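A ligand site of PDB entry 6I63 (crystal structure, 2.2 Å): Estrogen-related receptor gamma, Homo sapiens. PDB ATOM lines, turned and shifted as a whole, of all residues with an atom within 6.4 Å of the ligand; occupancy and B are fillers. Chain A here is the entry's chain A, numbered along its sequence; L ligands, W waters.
An oxygen (O2) of the ligand is in hydrogen-bond range of the side-chain carboxylate (OE2) of Glu 54, at 2.7 Å.
ND2 of Asn 125 sits at hydrogen-bond distance from O1 of the ligand.
The guanidinium group (NH2) of Arg 95 sits at hydrogen-bond distance from an oxygen (O2) of the ligand (3.1 Å).
Residues that only touch the ligand: Tyr 105, Phe 214, Ile 128, Leu 124, Met 85, Leu 88, Leu 47 and Ala 51.
Hydrophobic or aromatic side chains within 4 Å of the ligand: Leu 47, Ala 51, Met 85, Leu 88, Tyr 105, Leu 124, Ile 128 and Phe 214.
Within 4 Å of the ligand: Leu 47, Ala 51, Glu 54, Met 85, Leu 88, Arg 95, Tyr 105, Leu 124, Asn 125, Ile 128 and Phe 214.
The guanidinium group of Arg 95 sits at hydrogen-bond distance from the backbone carbonyl oxygen of Val 104 (2.9 Å).
The backbone carbonyl oxygen (O) of Gly 91 lies close to the guanidinium group (NH1) of Arg 95, 3.4 Å away.
The side-chain amide nitrogen (ND2) of Asn 125 is in hydrogen-bond range of the side-chain hydroxyl (OH) of Tyr 105.
The guanidinium group (NH2) of Arg 95 sits at hydrogen-bond distance from the backbone carbonyl oxygen (O) of Tyr 105 (3.0 Å).
Water W1 lies within hydrogen-bond range of O of Leu 88, OE1 of Glu 54, NH1 of Arg 95 and O2 of the ligand.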
ATOM      1  N   LEU A  44     -12.660 -33.970  17.791  1.00  0.00           N
ATOM      2  CA  LEU A  44     -11.960 -34.079  19.058  1.00  0.00           C
ATOM      3  C   LEU A  44     -10.812 -35.078  18.959  1.00  0.00           C
ATOM      4  O   LEU A  44      -9.756 -34.872  19.557  1.00  0.00           O
ATOM      5  CB  LEU A  44     -12.928 -34.488  20.172  1.00  0.00           C
ATOM      6  CG  LEU A  44     -13.990 -33.436  20.521  1.00  0.00           C
ATOM      7  CD1 LEU A  44     -14.949 -33.969  21.583  1.00  0.00           C
ATOM      8  CD2 LEU A  44     -13.363 -32.108  20.959  1.00  0.00           C
ATOM      9  N   LEU A  47      -8.064 -33.206  17.004  1.00  0.00           N
ATOM     10  CA  LEU A  47      -7.419 -32.175  17.828  1.00  0.00           C
ATOM     11  C   LEU A  47      -6.487 -32.787  18.863  1.00  0.00           C
ATOM     12  O   LEU A  47      -5.350 -32.325  19.027  1.00  0.00           O
ATOM     13  CB  LEU A  47      -8.471 -31.299  18.501  1.00  0.00           C
ATOM     14  CG  LEU A  47      -9.214 -30.350  17.551  1.00  0.00           C
ATOM     15  CD1 LEU A  47     -10.225 -29.560  18.337  1.00  0.00           C
ATOM     16  CD2 LEU A  47      -8.274 -29.391  16.867  1.00  0.00           C
ATOM     17  N   CYS A  48      -6.948 -33.832  19.552  1.00  0.00           N
ATOM     18  CA  CYS A  48      -6.151 -34.472  20.601  1.00  0.00           C
ATOM     19  C   CYS A  48      -4.928 -35.176  20.038  1.00  0.00           C
ATOM     20  O   CYS A  48      -3.881 -35.245  20.679  1.00  0.00           O
ATOM     21  CB  CYS A  48      -7.010 -35.459  21.388  1.00  0.00           C
ATOM     22  SG  CYS A  48      -8.171 -34.621  22.474  1.00  0.00           S
ATOM     23  N   LEU A  50      -3.399 -34.219  17.194  1.00  0.00           N
ATOM     24  CA  LEU A  50      -2.534 -33.116  16.815  1.00  0.00           C
ATOM     25  C   LEU A  50      -1.731 -32.600  18.029  1.00  0.00           C
ATOM     26  O   LEU A  50      -0.528 -32.365  17.926  1.00  0.00           O
ATOM     27  CB  LEU A  50      -3.366 -31.993  16.204  1.00  0.00           C
ATOM     28  CG  LEU A  50      -2.646 -30.708  15.811  1.00  0.00           C
ATOM     29  CD1 LEU A  50      -1.623 -30.990  14.721  1.00  0.00           C
ATOM     30  CD2 LEU A  50      -3.662 -29.665  15.323  1.00  0.00           C
ATOM     31  N   ALA A  51      -2.404 -32.441  19.160  1.00  0.00           N
ATOM     32  CA  ALA A  51      -1.787 -31.920  20.367  1.00  0.00           C
ATOM     33  C   ALA A  51      -0.710 -32.870  20.876  1.00  0.00           C
ATOM     34  O   ALA A  51       0.356 -32.435  21.327  1.00  0.00           O
ATOM     35  CB  ALA A  51      -2.834 -31.665  21.454  1.00  0.00           C
ATOM     36  N   GLU A  54       2.283 -32.410  18.783  1.00  0.00           N
ATOM     37  CA  GLU A  54       2.892 -31.104  19.060  1.00  0.00           C
ATOM     38  C   GLU A  54       3.637 -31.075  20.415  1.00  0.00           C
ATOM     39  O   GLU A  54       4.635 -30.379  20.560  1.00  0.00           O
ATOM     40  CB  GLU A  54       1.832 -30.011  19.056  1.00  0.00           C
ATOM     41  CG  GLU A  54       1.380 -29.607  17.667  1.00  0.00           C
ATOM     42  CD  GLU A  54       0.566 -28.337  17.702  1.00  0.00           C
ATOM     43  OE1 GLU A  54       1.182 -27.274  17.912  1.00  0.00           O
ATOM     44  OE2 GLU A  54      -0.671 -28.393  17.547  1.00  0.00           O
ATOM     45  N   TRP A  84       2.313 -26.549  29.192  1.00  0.00           N
ATOM     46  CA  TRP A  84       2.136 -27.113  27.853  1.00  0.00           C
ATOM     47  C   TRP A  84       0.870 -26.605  27.163  1.00  0.00           C
ATOM     48  O   TRP A  84       0.886 -26.282  25.965  1.00  0.00           O
ATOM     49  CB  TRP A  84       2.124 -28.653  27.900  1.00  0.00           C
ATOM     50  CG  TRP A  84       1.003 -29.261  28.683  1.00  0.00           C
ATOM     51  CD1 TRP A  84       0.984 -29.526  30.025  1.00  0.00           C
ATOM     52  CD2 TRP A  84      -0.279 -29.679  28.177  1.00  0.00           C
ATOM     53  NE1 TRP A  84      -0.224 -30.072  30.381  1.00  0.00           N
ATOM     54  CE2 TRP A  84      -1.014 -30.191  29.268  1.00  0.00           C
ATOM     55  CE3 TRP A  84      -0.873 -29.677  26.906  1.00  0.00           C
ATOM     56  CZ2 TRP A  84      -2.323 -30.691  29.143  1.00  0.00           C
ATOM     57  CZ3 TRP A  84      -2.167 -30.191  26.781  1.00  0.00           C
ATOM     58  CH2 TRP A  84      -2.875 -30.687  27.883  1.00  0.00           C
ATOM     59  N   MET A  85      -0.220 -26.489  27.911  1.00  0.00           N
ATOM     60  CA  MET A  85      -1.491 -26.073  27.331  1.00  0.00           C
ATOM     61  C   MET A  85      -1.431 -24.605  26.867  1.00  0.00           C
ATOM     62  O   MET A  85      -1.938 -24.270  25.790  1.00  0.00           O
ATOM     63  CB  MET A  85      -2.625 -26.311  28.313  1.00  0.00           C
ATOM     64  CG  MET A  85      -3.979 -25.836  27.798  1.00  0.00           C
ATOM     65  SD  MET A  85      -4.607 -26.784  26.386  1.00  0.00           S
ATOM     66  CE  MET A  85      -5.337 -28.189  27.249  1.00  0.00           C
ATOM     67  N   LEU A  88       0.518 -24.539  23.574  1.00  0.00           N
ATOM     68  CA  LEU A  88      -0.304 -25.000  22.456  1.00  0.00           C
ATOM     69  C   LEU A  88      -1.252 -23.896  22.013  1.00  0.00           C
ATOM     70  O   LEU A  88      -1.364 -23.609  20.816  1.00  0.00           O
ATOM     71  CB  LEU A  88      -1.104 -26.253  22.838  1.00  0.00           C
ATOM     72  CG  LEU A  88      -0.348 -27.583  22.928  1.00  0.00           C
ATOM     73  CD1 LEU A  88      -1.285 -28.688  23.420  1.00  0.00           C
ATOM     74  CD2 LEU A  88       0.248 -27.961  21.584  1.00  0.00           C
ATOM     75  N   ILE A  89      -1.920 -23.264  22.980  1.00  0.00           N
ATOM     76  CA  ILE A  89      -2.938 -22.278  22.662  1.00  0.00           C
ATOM     77  C   ILE A  89      -2.310 -21.023  22.052  1.00  0.00           C
ATOM     78  O   ILE A  89      -2.873 -20.423  21.130  1.00  0.00           O
ATOM     79  CB  ILE A  89      -3.787 -21.924  23.908  1.00  0.00           C
ATOM     80  CG1 ILE A  89      -4.740 -23.079  24.200  1.00  0.00           C
ATOM     81  CG2 ILE A  89      -4.603 -20.646  23.707  1.00  0.00           C
ATOM     82  CD1 ILE A  89      -5.391 -22.966  25.569  1.00  0.00           C
ATOM     83  N   GLY A  91       0.259 -20.973  20.200  1.00  0.00           N
ATOM     84  CA  GLY A  91       0.479 -21.403  18.843  1.00  0.00           C
ATOM     85  C   GLY A  91      -0.710 -21.212  17.930  1.00  0.00           C
ATOM     86  O   GLY A  91      -0.561 -20.642  16.838  1.00  0.00           O
ATOM     87  N   VAL A  92      -1.886 -21.679  18.347  1.00  0.00           N
ATOM     88  CA  VAL A  92      -3.042 -21.541  17.472  1.00  0.00           C
ATOM     89  C   VAL A  92      -3.448 -20.069  17.381  1.00  0.00           C
ATOM     90  O   VAL A  92      -3.866 -19.609  16.319  1.00  0.00           O
ATOM     91  CB  VAL A  92      -4.251 -22.440  17.923  1.00  0.00           C
ATOM     92  CG1 VAL A  92      -4.624 -22.203  19.355  1.00  0.00           C
ATOM     93  CG2 VAL A  92      -5.449 -22.201  17.005  1.00  0.00           C
ATOM     94  N   ARG A  95      -1.095 -18.529  14.730  1.00  0.00           N
ATOM     95  CA  ARG A  95      -1.451 -18.977  13.386  1.00  0.00           C
ATOM     96  C   ARG A  95      -2.740 -18.360  12.858  1.00  0.00           C
ATOM     97  O   ARG A  95      -2.991 -18.383  11.654  1.00  0.00           O
ATOM     98  CB  ARG A  95      -1.582 -20.500  13.341  1.00  0.00           C
ATOM     99  CG  ARG A  95      -0.280 -21.196  13.606  1.00  0.00           C
ATOM    100  CD  ARG A  95      -0.361 -22.684  13.318  1.00  0.00           C
ATOM    101  NE  ARG A  95      -1.205 -23.447  14.237  1.00  0.00           N
ATOM    102  CZ  ARG A  95      -0.810 -23.931  15.425  1.00  0.00           C
ATOM    103  NH1 ARG A  95       0.416 -23.705  15.871  1.00  0.00           N
ATOM    104  NH2 ARG A  95      -1.647 -24.644  16.174  1.00  0.00           N
ATOM    105  N   LEU A 103     -10.046 -20.384  13.530  1.00  0.00           N
ATOM    106  CA  LEU A 103      -8.909 -20.824  14.302  1.00  0.00           C
ATOM    107  C   LEU A 103      -8.088 -21.832  13.497  1.00  0.00           C
ATOM    108  O   LEU A 103      -8.598 -22.887  13.121  1.00  0.00           O
ATOM    109  CB  LEU A 103      -9.365 -21.413  15.649  1.00  0.00           C
ATOM    110  CG  LEU A 103      -9.917 -20.361  16.634  1.00  0.00           C
ATOM    111  CD1 LEU A 103     -10.357 -20.991  17.942  1.00  0.00           C
ATOM    112  CD2 LEU A 103      -8.862 -19.308  16.894  1.00  0.00           C
ATOM    113  N   VAL A 104      -6.832 -21.484  13.208  1.00  0.00           N
ATOM    114  CA  VAL A 104      -5.971 -22.318  12.381  1.00  0.00           C
ATOM    115  C   VAL A 104      -5.176 -23.271  13.256  1.00  0.00           C
ATOM    116  O   VAL A 104      -4.046 -22.974  13.653  1.00  0.00           O
ATOM    117  CB  VAL A 104      -4.987 -21.462  11.512  1.00  0.00           C
ATOM    118  CG1 VAL A 104      -4.100 -22.342  10.624  1.00  0.00           C
ATOM    119  CG2 VAL A 104      -5.771 -20.437  10.671  1.00  0.00           C
ATOM    120  N   TYR A 105      -5.766 -24.416  13.581  1.00  0.00           N
ATOM    121  CA  TYR A 105      -5.056 -25.449  14.329  1.00  0.00           C
ATOM    122  C   TYR A 105      -3.934 -26.031  13.491  1.00  0.00           C
ATOM    123  O   TYR A 105      -2.873 -26.379  14.010  1.00  0.00           O
ATOM    124  CB  TYR A 105      -6.023 -26.542  14.786  1.00  0.00           C
ATOM    125  CG  TYR A 105      -6.902 -26.047  15.906  1.00  0.00           C
ATOM    126  CD1 TYR A 105      -6.497 -26.193  17.236  1.00  0.00           C
ATOM    127  CD2 TYR A 105      -8.087 -25.372  15.642  1.00  0.00           C
ATOM    128  CE1 TYR A 105      -7.289 -25.707  18.271  1.00  0.00           C
ATOM    129  CE2 TYR A 105      -8.879 -24.886  16.677  1.00  0.00           C
ATOM    130  CZ  TYR A 105      -8.478 -25.052  17.980  1.00  0.00           C
ATOM    131  OH  TYR A 105      -9.248 -24.559  19.006  1.00  0.00           O
ATOM    132  N   MET A 111     -10.928 -24.222  12.069  1.00  0.00           N
ATOM    133  CA  MET A 111     -12.285 -24.310  12.626  1.00  0.00           C
ATOM    134  C   MET A 111     -13.001 -22.979  12.582  1.00  0.00           C
ATOM    135  O   MET A 111     -12.470 -21.945  13.008  1.00  0.00           O
ATOM    136  CB  MET A 111     -12.268 -24.813  14.082  1.00  0.00           C
ATOM    137  CG  MET A 111     -11.617 -26.167  14.254  1.00  0.00           C
ATOM    138  SD  MET A 111     -12.003 -26.912  15.855  1.00  0.00           S
ATOM    139  CE  MET A 111     -13.776 -27.016  15.741  1.00  0.00           C
ATOM    140  N   LEU A 121     -17.151 -26.952  21.349  1.00  0.00           N
ATOM    141  CA  LEU A 121     -15.970 -26.174  21.713  1.00  0.00           C
ATOM    142  C   LEU A 121     -16.209 -24.684  21.556  1.00  0.00           C
ATOM    143  O   LEU A 121     -15.258 -23.894  21.602  1.00  0.00           O
ATOM    144  CB  LEU A 121     -14.764 -26.593  20.858  1.00  0.00           C
ATOM    145  CG  LEU A 121     -14.077 -27.920  21.203  1.00  0.00           C
ATOM    146  CD1 LEU A 121     -13.000 -28.230  20.190  1.00  0.00           C
ATOM    147  CD2 LEU A 121     -13.501 -27.910  22.609  1.00  0.00           C
ATOM    148  N   LEU A 124     -14.966 -22.404  24.497  1.00  0.00           N
ATOM    149  CA  LEU A 124     -13.519 -22.461  24.626  1.00  0.00           C
ATOM    150  C   LEU A 124     -12.875 -21.756  23.430  1.00  0.00           C
ATOM    151  O   LEU A 124     -11.964 -20.918  23.595  1.00  0.00           O
ATOM    152  CB  LEU A 124     -13.076 -23.908  24.726  1.00  0.00           C
ATOM    153  CG  LEU A 124     -11.971 -24.261  25.706  1.00  0.00           C
ATOM    154  CD1 LEU A 124     -12.102 -23.457  27.002  1.00  0.00           C
ATOM    155  CD2 LEU A 124     -12.082 -25.743  25.997  1.00  0.00           C
ATOM    156  N   ASN A 125     -13.345 -22.074  22.225  1.00  0.00           N
ATOM    157  CA  ASN A 125     -12.816 -21.448  21.024  1.00  0.00           C
ATOM    158  C   ASN A 125     -13.147 -19.955  20.947  1.00  0.00           C
ATOM    159  O   ASN A 125     -12.391 -19.178  20.354  1.00  0.00           O
ATOM    160  CB  ASN A 125     -13.327 -22.165  19.765  1.00  0.00           C
ATOM    161  CG  ASN A 125     -12.570 -23.456  19.487  1.00  0.00           C
ATOM    162  OD1 ASN A 125     -12.763 -24.105  18.457  1.00  0.00           O
ATOM    163  ND2 ASN A 125     -11.697 -23.839  20.403  1.00  0.00           N
ATOM    164  N   ILE A 128     -10.440 -18.345  22.981  1.00  0.00           N
ATOM    165  CA  ILE A 128      -9.217 -18.274  22.180  1.00  0.00           C
ATOM    166  C   ILE A 128      -9.297 -17.127  21.161  1.00  0.00           C
ATOM    167  O   ILE A 128      -8.329 -16.396  20.970  1.00  0.00           O
ATOM    168  CB  ILE A 128      -8.927 -19.619  21.461  1.00  0.00           C
ATOM    169  CG1 ILE A 128      -8.682 -20.721  22.504  1.00  0.00           C
ATOM    170  CG2 ILE A 128      -7.732 -19.507  20.530  1.00  0.00           C
ATOM    171  CD1 ILE A 128      -8.423 -22.083  21.911  1.00  0.00           C
ATOM    172  N   ALA A 210      -9.470 -24.921  29.483  1.00  0.00           N
ATOM    173  CA  ALA A 210      -9.241 -25.953  28.466  1.00  0.00           C
ATOM    174  C   ALA A 210      -8.776 -27.266  29.092  1.00  0.00           C
ATOM    175  O   ALA A 210      -9.143 -28.344  28.628  1.00  0.00           O
ATOM    176  CB  ALA A 210      -8.218 -25.485  27.427  1.00  0.00           C
ATOM    177  N   PHE A 214     -11.006 -30.836  28.642  1.00  0.00           N
ATOM    178  CA  PHE A 214     -10.540 -32.048  28.002  1.00  0.00           C
ATOM    179  C   PHE A 214     -10.339 -33.155  29.006  1.00  0.00           C
ATOM    180  O   PHE A 214     -10.280 -34.317  28.644  1.00  0.00           O
ATOM    181  CB  PHE A 214      -9.261 -31.786  27.198  1.00  0.00           C
ATOM    182  CG  PHE A 214      -9.542 -31.182  25.861  1.00  0.00           C
ATOM    183  CD1 PHE A 214      -9.839 -31.988  24.778  1.00  0.00           C
ATOM    184  CD2 PHE A 214      -9.554 -29.801  25.675  1.00  0.00           C
ATOM    185  CE1 PHE A 214     -10.133 -31.442  23.540  1.00  0.00           C
ATOM    186  CE2 PHE A 214      -9.838 -29.244  24.435  1.00  0.00           C
ATOM    187  CZ  PHE A 214     -10.131 -30.060  23.374  1.00  0.00           C
ATOM    188  N   PHE A 229      -0.228 -36.997  25.695  1.00  0.00           N
ATOM    189  CA  PHE A 229      -1.305 -36.036  25.948  1.00  0.00           C
ATOM    190  C   PHE A 229      -2.019 -36.374  27.248  1.00  0.00           C
ATOM    191  O   PHE A 229      -2.256 -35.486  28.081  1.00  0.00           O
ATOM    192  CB  PHE A 229      -2.291 -36.014  24.772  1.00  0.00           C
ATOM    193  CG  PHE A 229      -3.434 -35.037  24.936  1.00  0.00           C
ATOM    194  CD1 PHE A 229      -3.259 -33.692  24.653  1.00  0.00           C
ATOM    195  CD2 PHE A 229      -4.687 -35.470  25.356  1.00  0.00           C
ATOM    196  CE1 PHE A 229      -4.308 -32.777  24.795  1.00  0.00           C
ATOM    197  CE2 PHE A 229      -5.746 -34.566  25.499  1.00  0.00           C
ATOM    198  CZ  PHE A 229      -5.557 -33.234  25.217  1.00  0.00           C
HETATM  199  O1  LIG L   1     -10.537 -24.911  22.387  1.00  0.00           O
HETATM  200  C1  LIG L   1      -9.496 -25.805  22.316  1.00  0.00           C
HETATM  201  C2  LIG L   1      -8.590 -25.902  23.371  1.00  0.00           C
HETATM  202  C3  LIG L   1      -7.527 -26.800  23.334  1.00  0.00           C
HETATM  203  C4  LIG L   1      -9.338 -26.621  21.204  1.00  0.00           C
HETATM  204  C5  LIG L   1      -8.276 -27.522  21.152  1.00  0.00           C
HETATM  205  C6  LIG L   1      -7.378 -27.611  22.207  1.00  0.00           C
HETATM  206  C7  LIG L   1      -6.236 -28.602  22.123  1.00  0.00           C
HETATM  207  C8  LIG L   1      -6.776 -29.983  21.726  1.00  0.00           C
HETATM  208  C9  LIG L   1      -5.513 -28.700  23.472  1.00  0.00           C
HETATM  209  C10 LIG L   1      -5.216 -28.077  21.114  1.00  0.00           C
HETATM  210  C11 LIG L   1      -4.750 -28.885  20.068  1.00  0.00           C
HETATM  211  C12 LIG L   1      -3.808 -28.383  19.182  1.00  0.00           C
HETATM  212  C13 LIG L   1      -4.736 -26.778  21.281  1.00  0.00           C
HETATM  213  C14 LIG L   1      -3.798 -26.281  20.403  1.00  0.00           C
HETATM  214  C15 LIG L   1      -3.328 -27.084  19.349  1.00  0.00           C
HETATM  215  O2  LIG L   1      -2.406 -26.588  18.487  1.00  0.00           O
HETATM  216  O   HOH W   1       0.187 -24.747  18.737  1.00  0.00           O
